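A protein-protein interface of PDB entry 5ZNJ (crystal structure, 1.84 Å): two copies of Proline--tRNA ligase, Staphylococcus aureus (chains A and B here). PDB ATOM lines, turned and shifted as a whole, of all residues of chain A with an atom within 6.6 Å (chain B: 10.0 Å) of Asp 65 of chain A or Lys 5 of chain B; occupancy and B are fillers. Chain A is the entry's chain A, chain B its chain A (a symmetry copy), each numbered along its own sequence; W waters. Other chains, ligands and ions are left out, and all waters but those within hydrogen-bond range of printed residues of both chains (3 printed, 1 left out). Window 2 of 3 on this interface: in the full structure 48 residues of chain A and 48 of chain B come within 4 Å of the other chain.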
ATOM      1  N   GLU A  60      -9.892 -19.581  -6.709  1.00  0.00           N
ATOM      2  CA  GLU A  60      -9.796 -19.704  -8.162  1.00  0.00           C
ATOM      3  C   GLU A  60      -8.674 -18.844  -8.742  1.00  0.00           C
ATOM      4  O   GLU A  60      -8.042 -19.236  -9.736  1.00  0.00           O
ATOM      5  CB  GLU A  60     -11.146 -19.382  -8.818  1.00  0.00           C
ATOM      6  CG  GLU A  60     -12.266 -20.346  -8.426  1.00  0.00           C
ATOM      7  CD  GLU A  60     -12.054 -21.780  -8.898  1.00  0.00           C
ATOM      8  OE1 GLU A  60     -11.290 -22.011  -9.858  1.00  0.00           O
ATOM      9  OE2 GLU A  60     -12.669 -22.684  -8.313  1.00  0.00           O
ATOM     10  N   MET A  61      -8.409 -17.689  -8.125  1.00  0.00           N
ATOM     11  CA  MET A  61      -7.246 -16.877  -8.507  1.00  0.00           C
ATOM     12  C   MET A  61      -5.936 -17.589  -8.164  1.00  0.00           C
ATOM     13  O   MET A  61      -5.036 -17.675  -9.007  1.00  0.00           O
ATOM     14  CB  MET A  61      -7.296 -15.481  -7.870  1.00  0.00           C
ATOM     15  CG  MET A  61      -8.392 -14.572  -8.421  1.00  0.00           C
ATOM     16  SD  MET A  61      -8.227 -14.125 -10.160  1.00  0.00           S
ATOM     17  CE  MET A  61      -9.229 -15.365 -10.982  1.00  0.00           C
ATOM     18  N   GLU A  62      -5.831 -18.128  -6.952  1.00  0.00           N
ATOM     19  CA  GLU A  62      -4.608 -18.849  -6.566  1.00  0.00           C
ATOM     20  C   GLU A  62      -4.337 -20.062  -7.468  1.00  0.00           C
ATOM     21  O   GLU A  62      -3.184 -20.346  -7.789  1.00  0.00           O
ATOM     22  CB  GLU A  62      -4.632 -19.270  -5.091  1.00  0.00           C
ATOM     23  CG  GLU A  62      -3.309 -19.888  -4.639  1.00  0.00           C
ATOM     24  CD  GLU A  62      -3.011 -19.724  -3.159  1.00  0.00           C
ATOM     25  OE1 GLU A  62      -3.943 -19.491  -2.358  1.00  0.00           O
ATOM     26  OE2 GLU A  62      -1.818 -19.837  -2.799  1.00  0.00           O
ATOM     27  N   ARG A  63      -5.400 -20.741  -7.893  1.00  0.00           N
ATOM     28  CA  ARG A  63      -5.302 -21.887  -8.812  1.00  0.00           C
ATOM     29  C   ARG A  63      -4.620 -21.567 -10.153  1.00  0.00           C
ATOM     30  O   ARG A  63      -3.986 -22.447 -10.746  1.00  0.00           O
ATOM     31  CB  ARG A  63      -6.693 -22.465  -9.068  1.00  0.00           C
ATOM     32  CG  ARG A  63      -6.703 -23.822  -9.744  1.00  0.00           C
ATOM     33  CD  ARG A  63      -8.123 -24.289 -10.012  1.00  0.00           C
ATOM     34  NE  ARG A  63      -8.182 -25.214 -11.142  1.00  0.00           N
ATOM     35  CZ  ARG A  63      -8.051 -24.872 -12.426  1.00  0.00           C
ATOM     36  NH1 ARG A  63      -7.845 -23.603 -12.789  1.00  0.00           N
ATOM     37  NH2 ARG A  63      -8.121 -25.812 -13.364  1.00  0.00           N
ATOM     38  N   ILE A  64      -4.756 -20.330 -10.632  1.00  0.00           N
ATOM     39  CA  ILE A  64      -4.106 -19.902 -11.878  1.00  0.00           C
ATOM     40  C   ILE A  64      -2.922 -18.951 -11.649  1.00  0.00           C
ATOM     41  O   ILE A  64      -2.521 -18.244 -12.566  1.00  0.00           O
ATOM     42  CB  ILE A  64      -5.121 -19.283 -12.873  1.00  0.00           C
ATOM     43  CG1 ILE A  64      -5.765 -17.992 -12.318  1.00  0.00           C
ATOM     44  CG2 ILE A  64      -6.187 -20.308 -13.229  1.00  0.00           C
ATOM     45  CD1 ILE A  64      -6.452 -17.157 -13.377  1.00  0.00           C
ATOM     46  N   ASP A  65      -2.358 -18.954 -10.440  1.00  0.00           N
ATOM     47  CA  ASP A  65      -1.242 -18.068 -10.069  1.00  0.00           C
ATOM     48  C   ASP A  65      -1.526 -16.584 -10.286  1.00  0.00           C
ATOM     49  O   ASP A  65      -0.652 -15.834 -10.712  1.00  0.00           O
ATOM     50  CB  ASP A  65       0.048 -18.492 -10.797  1.00  0.00           C
ATOM     51  CG  ASP A  65       0.483 -19.887 -10.426  1.00  0.00           C
ATOM     52  OD1 ASP A  65       0.439 -20.204  -9.227  1.00  0.00           O
ATOM     53  OD2 ASP A  65       0.884 -20.660 -11.321  1.00  0.00           O
ATOM     54  N   SER A  66      -2.758 -16.170  -9.988  1.00  0.00           N
ATOM     55  CA  SER A  66      -3.115 -14.752  -9.953  1.00  0.00           C
ATOM     56  C   SER A  66      -2.975 -14.343  -8.490  1.00  0.00           C
ATOM     57  O   SER A  66      -3.692 -14.861  -7.639  1.00  0.00           O
ATOM     58  CB  SER A  66      -4.537 -14.542 -10.469  1.00  0.00           C
ATOM     59  OG  SER A  66      -4.965 -13.199 -10.298  1.00  0.00           O
ATOM     60  N   VAL A  67      -2.041 -13.431  -8.208  1.00  0.00           N
ATOM     61  CA  VAL A  67      -1.566 -13.181  -6.846  1.00  0.00           C
ATOM     62  C   VAL A  67      -2.193 -11.916  -6.242  1.00  0.00           C
ATOM     63  O   VAL A  67      -2.114 -10.841  -6.839  1.00  0.00           O
ATOM     64  CB  VAL A  67      -0.027 -13.088  -6.844  1.00  0.00           C
ATOM     65  CG1 VAL A  67       0.503 -12.806  -5.450  1.00  0.00           C
ATOM     66  CG2 VAL A  67       0.568 -14.395  -7.367  1.00  0.00           C
ATOM     67  N   GLN A 127      11.535 -12.727 -15.319  1.00  0.00           N
ATOM     68  CA  GLN A 127      10.520 -12.509 -14.276  1.00  0.00           C
ATOM     69  C   GLN A 127       9.062 -12.663 -14.746  1.00  0.00           C
ATOM     70  O   GLN A 127       8.147 -12.589 -13.923  1.00  0.00           O
ATOM     71  CB  GLN A 127      10.690 -11.110 -13.679  1.00  0.00           C
ATOM     72  CG  GLN A 127      12.056 -10.840 -13.067  1.00  0.00           C
ATOM     73  CD  GLN A 127      12.222  -9.385 -12.684  1.00  0.00           C
ATOM     74  OE1 GLN A 127      12.436  -8.536 -13.543  1.00  0.00           O
ATOM     75  NE2 GLN A 127      12.104  -9.085 -11.396  1.00  0.00           N
ATOM     76  N   PRO A 129       5.786 -14.637 -16.941  1.00  0.00           N
ATOM     77  CA  PRO A 129       4.680 -13.718 -16.647  1.00  0.00           C
ATOM     78  C   PRO A 129       4.401 -13.477 -15.155  1.00  0.00           C
ATOM     79  O   PRO A 129       4.852 -14.235 -14.292  1.00  0.00           O
ATOM     80  CB  PRO A 129       3.478 -14.419 -17.284  1.00  0.00           C
ATOM     81  CG  PRO A 129       3.802 -15.869 -17.166  1.00  0.00           C
ATOM     82  CD  PRO A 129       5.296 -15.972 -17.334  1.00  0.00           C
ATOM     83  N   MET A 130       3.641 -12.416 -14.892  1.00  0.00           N
ATOM     84  CA  MET A 130       3.218 -12.034 -13.550  1.00  0.00           C
ATOM     85  C   MET A 130       1.764 -11.587 -13.605  1.00  0.00           C
ATOM     86  O   MET A 130       1.419 -10.759 -14.443  1.00  0.00           O
ATOM     87  CB  MET A 130       4.073 -10.860 -13.070  1.00  0.00           C
ATOM     88  CG  MET A 130       3.734 -10.319 -11.688  1.00  0.00           C
ATOM     89  SD  MET A 130       3.959 -11.546 -10.396  1.00  0.00           S
ATOM     90  CE  MET A 130       5.752 -11.724 -10.444  1.00  0.00           C
ATOM     91  N   THR A 131       0.936 -12.103 -12.692  1.00  0.00           N
ATOM     92  CA  THR A 131      -0.481 -11.750 -12.612  1.00  0.00           C
ATOM     93  C   THR A 131      -0.813 -11.305 -11.193  1.00  0.00           C
ATOM     94  O   THR A 131      -0.499 -12.008 -10.238  1.00  0.00           O
ATOM     95  CB  THR A 131      -1.376 -12.943 -13.007  1.00  0.00           C
ATOM     96  OG1 THR A 131      -1.052 -13.349 -14.336  1.00  0.00           O
ATOM     97  CG2 THR A 131      -2.857 -12.573 -12.966  1.00  0.00           C
ATOM     98  N   LEU A 132      -1.428 -10.127 -11.077  1.00  0.00           N
ATOM     99  CA  LEU A 132      -1.809  -9.550  -9.792  1.00  0.00           C
ATOM    100  C   LEU A 132      -3.301  -9.248  -9.797  1.00  0.00           C
ATOM    101  O   LEU A 132      -3.857  -8.896 -10.840  1.00  0.00           O
ATOM    102  CB  LEU A 132      -1.033  -8.256  -9.546  1.00  0.00           C
ATOM    103  CG  LEU A 132       0.494  -8.334  -9.627  1.00  0.00           C
ATOM    104  CD1 LEU A 132       1.103  -6.940  -9.572  1.00  0.00           C
ATOM    105  CD2 LEU A 132       1.040  -9.215  -8.515  1.00  0.00           C
ATOM    106  N   MET B   1       2.758 -21.487  -3.297  1.00  0.00           N
ATOM    107  CA  MET B   1       3.043 -20.620  -4.473  1.00  0.00           C
ATOM    108  C   MET B   1       4.506 -20.741  -4.867  1.00  0.00           C
ATOM    109  O   MET B   1       5.386 -20.788  -4.004  1.00  0.00           O
ATOM    110  CB  MET B   1       2.741 -19.154  -4.157  1.00  0.00           C
ATOM    111  CG  MET B   1       1.273 -18.770  -4.190  1.00  0.00           C
ATOM    112  SD  MET B   1       0.525 -18.808  -5.835  1.00  0.00           S
ATOM    113  CE  MET B   1       1.833 -18.157  -6.865  1.00  0.00           C
ATOM    114  N   LYS B   2       4.758 -20.785  -6.172  1.00  0.00           N
ATOM    115  CA  LYS B   2       6.117 -20.715  -6.702  1.00  0.00           C
ATOM    116  C   LYS B   2       6.527 -19.249  -6.713  1.00  0.00           C
ATOM    117  O   LYS B   2       5.820 -18.411  -7.278  1.00  0.00           O
ATOM    118  CB  LYS B   2       6.198 -21.307  -8.104  1.00  0.00           C
ATOM    119  CG  LYS B   2       6.144 -22.824  -8.095  1.00  0.00           C
ATOM    120  CD  LYS B   2       6.163 -23.385  -9.505  1.00  0.00           C
ATOM    121  CE  LYS B   2       6.402 -24.887  -9.499  1.00  0.00           C
ATOM    122  NZ  LYS B   2       5.203 -25.640  -9.032  1.00  0.00           N
ATOM    123  N   GLN B   3       7.671 -18.957  -6.097  1.00  0.00           N
ATOM    124  CA  GLN B   3       8.169 -17.587  -5.951  1.00  0.00           C
ATOM    125  C   GLN B   3       8.430 -16.880  -7.292  1.00  0.00           C
ATOM    126  O   GLN B   3       8.311 -15.658  -7.376  1.00  0.00           O
ATOM    127  CB  GLN B   3       9.433 -17.586  -5.092  1.00  0.00           C
ATOM    128  CG  GLN B   3       9.841 -16.219  -4.567  1.00  0.00           C
ATOM    129  CD  GLN B   3      10.858 -16.305  -3.439  1.00  0.00           C
ATOM    130  OE1 GLN B   3      10.881 -17.275  -2.682  1.00  0.00           O
ATOM    131  NE2 GLN B   3      11.694 -15.282  -3.314  1.00  0.00           N
ATOM    132  N   SER B   4       8.737 -17.647  -8.343  1.00  0.00           N
ATOM    133  CA  SER B   4       8.829 -17.104  -9.706  1.00  0.00           C
ATOM    134  C   SER B   4       7.535 -16.421 -10.190  1.00  0.00           C
ATOM    135  O   SER B   4       7.588 -15.576 -11.083  1.00  0.00           O
ATOM    136  CB  SER B   4       9.230 -18.197 -10.705  1.00  0.00           C
ATOM    137  OG  SER B   4       8.248 -19.215 -10.773  1.00  0.00           O
ATOM    138  N   LYS B   5       6.392 -16.780  -9.603  1.00  0.00           N
ATOM    139  CA  LYS B   5       5.096 -16.164  -9.939  1.00  0.00           C
ATOM    140  C   LYS B   5       4.553 -15.150  -8.917  1.00  0.00           C
ATOM    141  O   LYS B   5       3.445 -14.630  -9.094  1.00  0.00           O
ATOM    142  CB  LYS B   5       4.079 -17.281 -10.208  1.00  0.00           C
ATOM    143  CG  LYS B   5       4.251 -17.878 -11.597  1.00  0.00           C
ATOM    144  CD  LYS B   5       4.046 -19.377 -11.620  1.00  0.00           C
ATOM    145  CE  LYS B   5       4.295 -19.938 -13.015  1.00  0.00           C
ATOM    146  NZ  LYS B   5       4.986 -21.256 -12.951  1.00  0.00           N
ATOM    147  N   VAL B   6       5.335 -14.836  -7.883  1.00  0.00           N
ATOM    148  CA  VAL B   6       4.929 -13.896  -6.836  1.00  0.00           C
ATOM    149  C   VAL B   6       5.785 -12.640  -6.935  1.00  0.00           C
ATOM    150  O   VAL B   6       7.020 -12.716  -6.882  1.00  0.00           O
ATOM    151  CB  VAL B   6       5.081 -14.494  -5.416  1.00  0.00           C
ATOM    152  CG1 VAL B   6       4.532 -13.543  -4.357  1.00  0.00           C
ATOM    153  CG2 VAL B   6       4.366 -15.827  -5.313  1.00  0.00           C
ATOM    154  N   PHE B   7       5.121 -11.486  -7.055  1.00  0.00           N
ATOM    155  CA  PHE B   7       5.806 -10.197  -7.117  1.00  0.00           C
ATOM    156  C   PHE B   7       6.392  -9.823  -5.748  1.00  0.00           C
ATOM    157  O   PHE B   7       5.647  -9.537  -4.808  1.00  0.00           O
ATOM    158  CB  PHE B   7       4.830  -9.118  -7.605  1.00  0.00           C
ATOM    159  CG  PHE B   7       5.463  -7.783  -7.847  1.00  0.00           C
ATOM    160  CD1 PHE B   7       6.381  -7.610  -8.885  1.00  0.00           C
ATOM    161  CD2 PHE B   7       5.135  -6.682  -7.056  1.00  0.00           C
ATOM    162  CE1 PHE B   7       6.965  -6.371  -9.115  1.00  0.00           C
ATOM    163  CE2 PHE B   7       5.713  -5.445  -7.283  1.00  0.00           C
ATOM    164  CZ  PHE B   7       6.631  -5.287  -8.315  1.00  0.00           C
ATOM    165  N   ILE B   8       7.723  -9.860  -5.634  1.00  0.00           N
ATOM    166  CA  ILE B   8       8.419  -9.518  -4.379  1.00  0.00           C
ATOM    167  C   ILE B   8       9.640  -8.655  -4.714  1.00  0.00           C
ATOM    168  O   ILE B   8      10.761  -9.181  -4.801  1.00  0.00           O
ATOM    169  CB  ILE B   8       8.862 -10.767  -3.562  1.00  0.00           C
ATOM    170  CG1 ILE B   8       7.750 -11.823  -3.467  1.00  0.00           C
ATOM    171  CG2 ILE B   8       9.306 -10.334  -2.167  1.00  0.00           C
ATOM    172  CD1 ILE B   8       8.161 -13.109  -2.771  1.00  0.00           C
ATOM    173  N   PRO B  44       2.099  -8.552  -2.635  1.00  0.00           N
ATOM    174  CA  PRO B  44       1.545  -9.868  -2.311  1.00  0.00           C
ATOM    175  C   PRO B  44       1.766 -10.393  -0.900  1.00  0.00           C
ATOM    176  O   PRO B  44       0.813 -10.843  -0.271  1.00  0.00           O
ATOM    177  CB  PRO B  44       2.216 -10.770  -3.335  1.00  0.00           C
ATOM    178  CG  PRO B  44       2.276  -9.897  -4.541  1.00  0.00           C
ATOM    179  CD  PRO B  44       2.683  -8.557  -3.992  1.00  0.00           C
ATOM    180  N   LEU B  45       2.997 -10.316  -0.398  1.00  0.00           N
ATOM    181  CA  LEU B  45       3.283 -10.808   0.956  1.00  0.00           C
ATOM    182  C   LEU B  45       2.564 -10.018   2.058  1.00  0.00           C
ATOM    183  O   LEU B  45       2.063 -10.618   3.008  1.00  0.00           O
ATOM    184  CB  LEU B  45       4.797 -10.854   1.227  1.00  0.00           C
ATOM    185  CG  LEU B  45       5.622 -11.848   0.399  1.00  0.00           C
ATOM    186  CD1 LEU B  45       7.072 -11.871   0.856  1.00  0.00           C
ATOM    187  CD2 LEU B  45       5.053 -13.247   0.455  1.00  0.00           C
ATOM    188  N   ARG B  48      -1.160 -11.038   2.171  1.00  0.00           N
ATOM    189  CA  ARG B  48      -1.343 -12.304   2.898  1.00  0.00           C
ATOM    190  C   ARG B  48      -1.295 -12.099   4.425  1.00  0.00           C
ATOM    191  O   ARG B  48      -2.131 -12.635   5.148  1.00  0.00           O
ATOM    192  CB  ARG B  48      -0.325 -13.352   2.440  1.00  0.00           C
ATOM    193  CG  ARG B  48      -0.510 -13.780   0.985  1.00  0.00           C
ATOM    194  CD  ARG B  48       0.520 -14.810   0.544  1.00  0.00           C
ATOM    195  NE  ARG B  48       0.225 -16.107   1.139  1.00  0.00           N
ATOM    196  CZ  ARG B  48      -0.521 -17.070   0.595  1.00  0.00           C
ATOM    197  NH1 ARG B  48      -1.070 -16.946  -0.620  1.00  0.00           N
ATOM    198  NH2 ARG B  48      -0.710 -18.196   1.273  1.00  0.00           N
ATOM    199  N   PHE B 470       3.610 -16.963   4.427  1.00  0.00           N
ATOM    200  CA  PHE B 470       3.717 -18.384   4.162  1.00  0.00           C
ATOM    201  C   PHE B 470       4.377 -19.052   5.369  1.00  0.00           C
ATOM    202  O   PHE B 470       5.101 -18.411   6.128  1.00  0.00           O
ATOM    203  CB  PHE B 470       4.563 -18.624   2.914  1.00  0.00           C
ATOM    204  CG  PHE B 470       3.945 -18.132   1.642  1.00  0.00           C
ATOM    205  CD1 PHE B 470       3.135 -18.965   0.877  1.00  0.00           C
ATOM    206  CD2 PHE B 470       4.219 -16.854   1.166  1.00  0.00           C
ATOM    207  CE1 PHE B 470       2.582 -18.521  -0.315  1.00  0.00           C
ATOM    208  CE2 PHE B 470       3.661 -16.404  -0.025  1.00  0.00           C
ATOM    209  CZ  PHE B 470       2.849 -17.239  -0.768  1.00  0.00           C
ATOM    210  N   ASP B 489      10.675 -29.976  -6.287  1.00  0.00           N
ATOM    211  CA  ASP B 489       9.329 -30.121  -6.876  1.00  0.00           C
ATOM    212  C   ASP B 489       8.479 -31.111  -6.083  1.00  0.00           C
ATOM    213  O   ASP B 489       7.320 -30.831  -5.771  1.00  0.00           O
ATOM    214  CB  ASP B 489       9.401 -30.569  -8.346  1.00  0.00           C
ATOM    215  CG  ASP B 489       9.842 -29.457  -9.286  1.00  0.00           C
ATOM    216  OD1 ASP B 489       9.962 -28.289  -8.855  1.00  0.00           O
ATOM    217  OD2 ASP B 489      10.076 -29.756 -10.477  1.00  0.00           O
ATOM    218  N   TYR B 492       7.624 -29.736  -2.540  1.00  0.00           N
ATOM    219  CA  TYR B 492       6.567 -28.729  -2.691  1.00  0.00           C
ATOM    220  C   TYR B 492       5.181 -29.376  -2.704  1.00  0.00           C
ATOM    221  O   TYR B 492       4.304 -28.982  -1.936  1.00  0.00           O
ATOM    222  CB  TYR B 492       6.778 -27.911  -3.962  1.00  0.00           C
ATOM    223  CG  TYR B 492       5.751 -26.821  -4.179  1.00  0.00           C
ATOM    224  CD1 TYR B 492       5.582 -25.801  -3.244  1.00  0.00           C
ATOM    225  CD2 TYR B 492       4.950 -26.804  -5.325  1.00  0.00           C
ATOM    226  CE1 TYR B 492       4.646 -24.792  -3.441  1.00  0.00           C
ATOM    227  CE2 TYR B 492       4.013 -25.801  -5.531  1.00  0.00           C
ATOM    228  CZ  TYR B 492       3.863 -24.797  -4.588  1.00  0.00           C
ATOM    229  OH  TYR B 492       2.934 -23.798  -4.791  1.00  0.00           O
ATOM    230  N   ASN B 496       2.788 -28.560   0.524  1.00  0.00           N
ATOM    231  CA  ASN B 496       1.853 -27.462   0.214  1.00  0.00           C
ATOM    232  C   ASN B 496       0.361 -27.816   0.376  1.00  0.00           C
ATOM    233  O   ASN B 496      -0.497 -27.041  -0.038  1.00  0.00           O
ATOM    234  CB  ASN B 496       2.129 -26.911  -1.196  1.00  0.00           C
ATOM    235  CG  ASN B 496       1.590 -25.494  -1.408  1.00  0.00           C
ATOM    236  OD1 ASN B 496       1.679 -24.635  -0.524  1.00  0.00           O
ATOM    237  ND2 ASN B 496       1.044 -25.240  -2.595  1.00  0.00           N
ATOM    238  N   VAL B 501       3.389 -23.098   1.402  1.00  0.00           N
ATOM    239  CA  VAL B 501       4.805 -23.116   1.086  1.00  0.00           C
ATOM    240  C   VAL B 501       5.095 -22.071   0.026  1.00  0.00           C
ATOM    241  O   VAL B 501       4.459 -22.058  -1.029  1.00  0.00           O
ATOM    242  CB  VAL B 501       5.251 -24.505   0.565  1.00  0.00           C
ATOM    243  CG1 VAL B 501       6.738 -24.511   0.236  1.00  0.00           C
ATOM    244  CG2 VAL B 501       4.944 -25.580   1.596  1.00  0.00           C
ATOM    245  N   LEU B 502       6.056 -21.202   0.310  1.00  0.00           N
ATOM    246  CA  LEU B 502       6.659 -20.380  -0.718  1.00  0.00           C
ATOM    247  C   LEU B 502       7.848 -21.176  -1.243  1.00  0.00           C
ATOM    248  O   LEU B 502       8.774 -21.470  -0.500  1.00  0.00           O
ATOM    249  CB  LEU B 502       7.106 -19.029  -0.165  1.00  0.00           C
ATOM    250  CG  LEU B 502       7.688 -18.032  -1.171  1.00  0.00           C
ATOM    251  CD1 LEU B 502       6.724 -17.711  -2.311  1.00  0.00           C
ATOM    252  CD2 LEU B 502       8.104 -16.758  -0.454  1.00  0.00           C
ATOM    253  N   TYR B 503       7.794 -21.537  -2.520  1.00  0.00           N
ATOM    254  CA  TYR B 503       8.831 -22.349  -3.157  1.00  0.00           C
ATOM    255  C   TYR B 503       9.703 -21.452  -4.018  1.00  0.00           C
ATOM    256  O   TYR B 503       9.275 -21.006  -5.085  1.00  0.00           O
ATOM    257  CB  TYR B 503       8.167 -23.452  -3.988  1.00  0.00           C
ATOM    258  CG  TYR B 503       9.063 -24.314  -4.872  1.00  0.00           C
ATOM    259  CD1 TYR B 503      10.447 -24.433  -4.656  1.00  0.00           C
ATOM    260  CD2 TYR B 503       8.501 -25.058  -5.912  1.00  0.00           C
ATOM    261  CE1 TYR B 503      11.234 -25.240  -5.474  1.00  0.00           C
ATOM    262  CE2 TYR B 503       9.282 -25.871  -6.727  1.00  0.00           C
ATOM    263  CZ  TYR B 503      10.645 -25.959  -6.507  1.00  0.00           C
ATOM    264  OH  TYR B 503      11.414 -26.772  -7.326  1.00  0.00           O
ATOM    265  N   ASP B 504      10.923 -21.182  -3.557  1.00  0.00           N
ATOM    266  CA  ASP B 504      11.858 -20.416  -4.364  1.00  0.00           C
ATOM    267  C   ASP B 504      12.462 -21.309  -5.451  1.00  0.00           C
ATOM    268  O   ASP B 504      13.551 -21.892  -5.302  1.00  0.00           O
ATOM    269  CB  ASP B 504      12.935 -19.715  -3.525  1.00  0.00           C
ATOM    270  CG  ASP B 504      13.595 -18.576  -4.281  1.00  0.00           C
ATOM    271  OD1 ASP B 504      13.359 -18.447  -5.503  1.00  0.00           O
ATOM    272  OD2 ASP B 504      14.342 -17.791  -3.668  1.00  0.00           O
ATOM    273  N   ASP B 505      11.715 -21.375  -6.547  1.00  0.00           N
ATOM    274  CA  ASP B 505      12.059 -22.134  -7.744  1.00  0.00           C
ATOM    275  C   ASP B 505      12.876 -21.326  -8.764  1.00  0.00           C
ATOM    276  O   ASP B 505      13.135 -21.810  -9.867  1.00  0.00           O
ATOM    277  CB  ASP B 505      10.760 -22.602  -8.413  1.00  0.00           C
ATOM    278  CG  ASP B 505       9.917 -21.441  -8.941  1.00  0.00           C
ATOM    279  OD1 ASP B 505       9.879 -20.368  -8.296  1.00  0.00           O
ATOM    280  OD2 ASP B 505       9.285 -21.603  -9.995  1.00  0.00           O
ATOM    281  N   ARG B 506      13.268 -20.102  -8.414  1.00  0.00           N
ATOM    282  CA  ARG B 506      13.854 -19.186  -9.383  1.00  0.00           C
ATOM    283  C   ARG B 506      15.238 -19.624  -9.836  1.00  0.00           C
ATOM    284  O   ARG B 506      15.966 -20.288  -9.089  1.00  0.00           O
ATOM    285  CB  ARG B 506      13.967 -17.783  -8.799  1.00  0.00           C
ATOM    286  CG  ARG B 506      12.636 -17.106  -8.506  1.00  0.00           C
ATOM    287  CD  ARG B 506      12.882 -15.737  -7.900  1.00  0.00           C
ATOM    288  NE  ARG B 506      13.574 -15.842  -6.611  1.00  0.00           N
ATOM    289  CZ  ARG B 506      14.204 -14.851  -5.976  1.00  0.00           C
ATOM    290  NH1 ARG B 506      14.250 -13.619  -6.481  1.00  0.00           N
ATOM    291  NH2 ARG B 506      14.797 -15.100  -4.804  1.00  0.00           N
ATOM    292  N   GLN B 507      15.580 -19.242 -11.062  1.00  0.00           N
ATOM    293  CA  GLN B 507      16.936 -19.370 -11.570  1.00  0.00           C
ATOM    294  C   GLN B 507      17.685 -18.118 -11.113  1.00  0.00           C
ATOM    295  O   GLN B 507      17.811 -17.136 -11.848  1.00  0.00           O
ATOM    296  CB  GLN B 507      16.933 -19.527 -13.097  1.00  0.00           C
ATOM    297  CG  GLN B 507      18.214 -20.128 -13.652  1.00  0.00           C
ATOM    298  CD  GLN B 507      18.350 -21.607 -13.324  1.00  0.00           C
ATOM    299  OE1 GLN B 507      19.003 -21.970 -12.348  1.00  0.00           O
ATOM    300  NE2 GLN B 507      17.713 -22.464 -14.124  1.00  0.00           N
HETATM  301  O   HOH W   1       6.895 -16.037 -13.972  1.00  0.00           O
HETATM  302  O   HOH W   2       1.781 -14.561 -11.278  1.00  0.00           O
HETATM  303  O   HOH W   3       2.737 -21.291  -7.983  1.00  0.00           O
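The side-chain sulfur of Met 130 of chain A lies close to the backbone NH of Phe 7 of chain B. The side-chain sulfur (SD) of Met 1 of chain B lies close to the side-chain carboxylate (OD1) of Asp 65 of chain A (3.7 Å). The backbone carbonyl oxygen (O) of Lys 5 of chain B lies close to the side-chain sulfur (SD) of Met 130 of chain A, 3.4 Å away. OE2 of Glu 62 of chain A is in salt-bridge range of NH1 of Arg 48 of chain B (3.7 Å).
The backbone NH (N) of Val 67 of chain A sits at hydrogen-bond distance from the backbone carbonyl oxygen (O) of Thr 131 of chain A (2.9 Å). The backbone NH of Met 1 of chain B sits at hydrogen-bond distance from the backbone carbonyl oxygen of Val 501 of chain B, at 2.9 Å. N of Met 1 of chain B is in hydrogen-bond range of OH of Tyr 492 of chain B (2.8 Å). O of Met 1 of chain B sits at hydrogen-bond distance from N of Tyr 503 of chain B (2.9 Å).
Among the printed residues, merely in contact across the chains: Val 67 of chain A with Lys 5 of chain B (3.4 Å), Val 67 of chain A with Pro 44 of chain B (3.4 Å), Asp 65 of chain A with Lys 5 of chain B (3.4 Å), Glu 62 of chain A with Met 1 of chain B (3.6 Å), Met 130 of chain A with Val 6 of chain B (3.6 Å) and Leu 132 of chain A with Phe 7 of chain B (3.9 Å).
Printed residues of chain B within 4 Å of Asp 65 of chain A: Met 1 (3.4 Å) and Lys 5 (3.4 Å). Lys 5 of chain B touches just these residues of chain A: Asp 65 (3.4 Å), Val 67 (3.4 Å) and Met 130 (3.4 Å). No residue of chain B comes within 4 Å of Ser 66 of chain A. No residue of chain B comes within 4 Å of Thr 131 of chain A. Printed residues of chain A within 4 Å of Val 6 of chain B: Met 130. Printed residues of chain A within 4 Å of Pro 44 of chain B: Val 67. Of the printed residues of chain B, Val 67 of chain A touches Lys 5 (3.4 Å) and Pro 44 (3.4 Å). Of the printed residues of chain B, Leu 132 of chain A touches Phe 7 (3.9 Å). Of the printed residues of chain B, Glu 62 of chain A touches Met 1 (3.6 Å) and Arg 48 (3.7 Å). Gln 507 of chain B touches none of the printed residues of chain A. The nearest printed residue of chain B that does not touch Asp 65 of chain A is Lys 2 of chain B (5.3 Å). The nearest printed residue of chain B that does not touch Met 130 of chain A is Ser 4 of chain B (4.3 Å).
Of the 13 printed residues of chain A, 5 touch a printed residue of chain B. Along chain A the printed residues that touch a printed residue of chain B span positions 62 to 132. Hydrophobic or aromatic side chains of chain B that line the printed part of chain A: Met 1, Phe 7 and Pro 44. Among the printed residues, Asp or Glu carboxylates within 4 Å of a Lys or Arg side-chain nitrogen of the other chain: Glu 62 of chain A with Arg 48 of chain B (3.7 Å).
No position is printed for both chains. Of the 10 pairs that touch across the chains among the printed residues, none has its exchanged pair printed and touching as well.
Water W1 bridges the backbone carbonyl oxygen of Pro 129 of chain A (2.7 Å) and the backbone carbonyl oxygen of Ser 4 of chain B (3.0 Å). Water W2 lies within hydrogen-bond range of the backbone carbonyl oxygen of Lys 5 of chain B, the backbone carbonyl oxygen of Asp 65 of chain A and the backbone NH of Thr 131 of chain A. Water W3 lies within hydrogen-bond range of the backbone NH (N) of Lys 2 of chain B (2.8 Å) and the side-chain carboxylate (OD1) of Asp 65 of chain A (2.8 Å).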
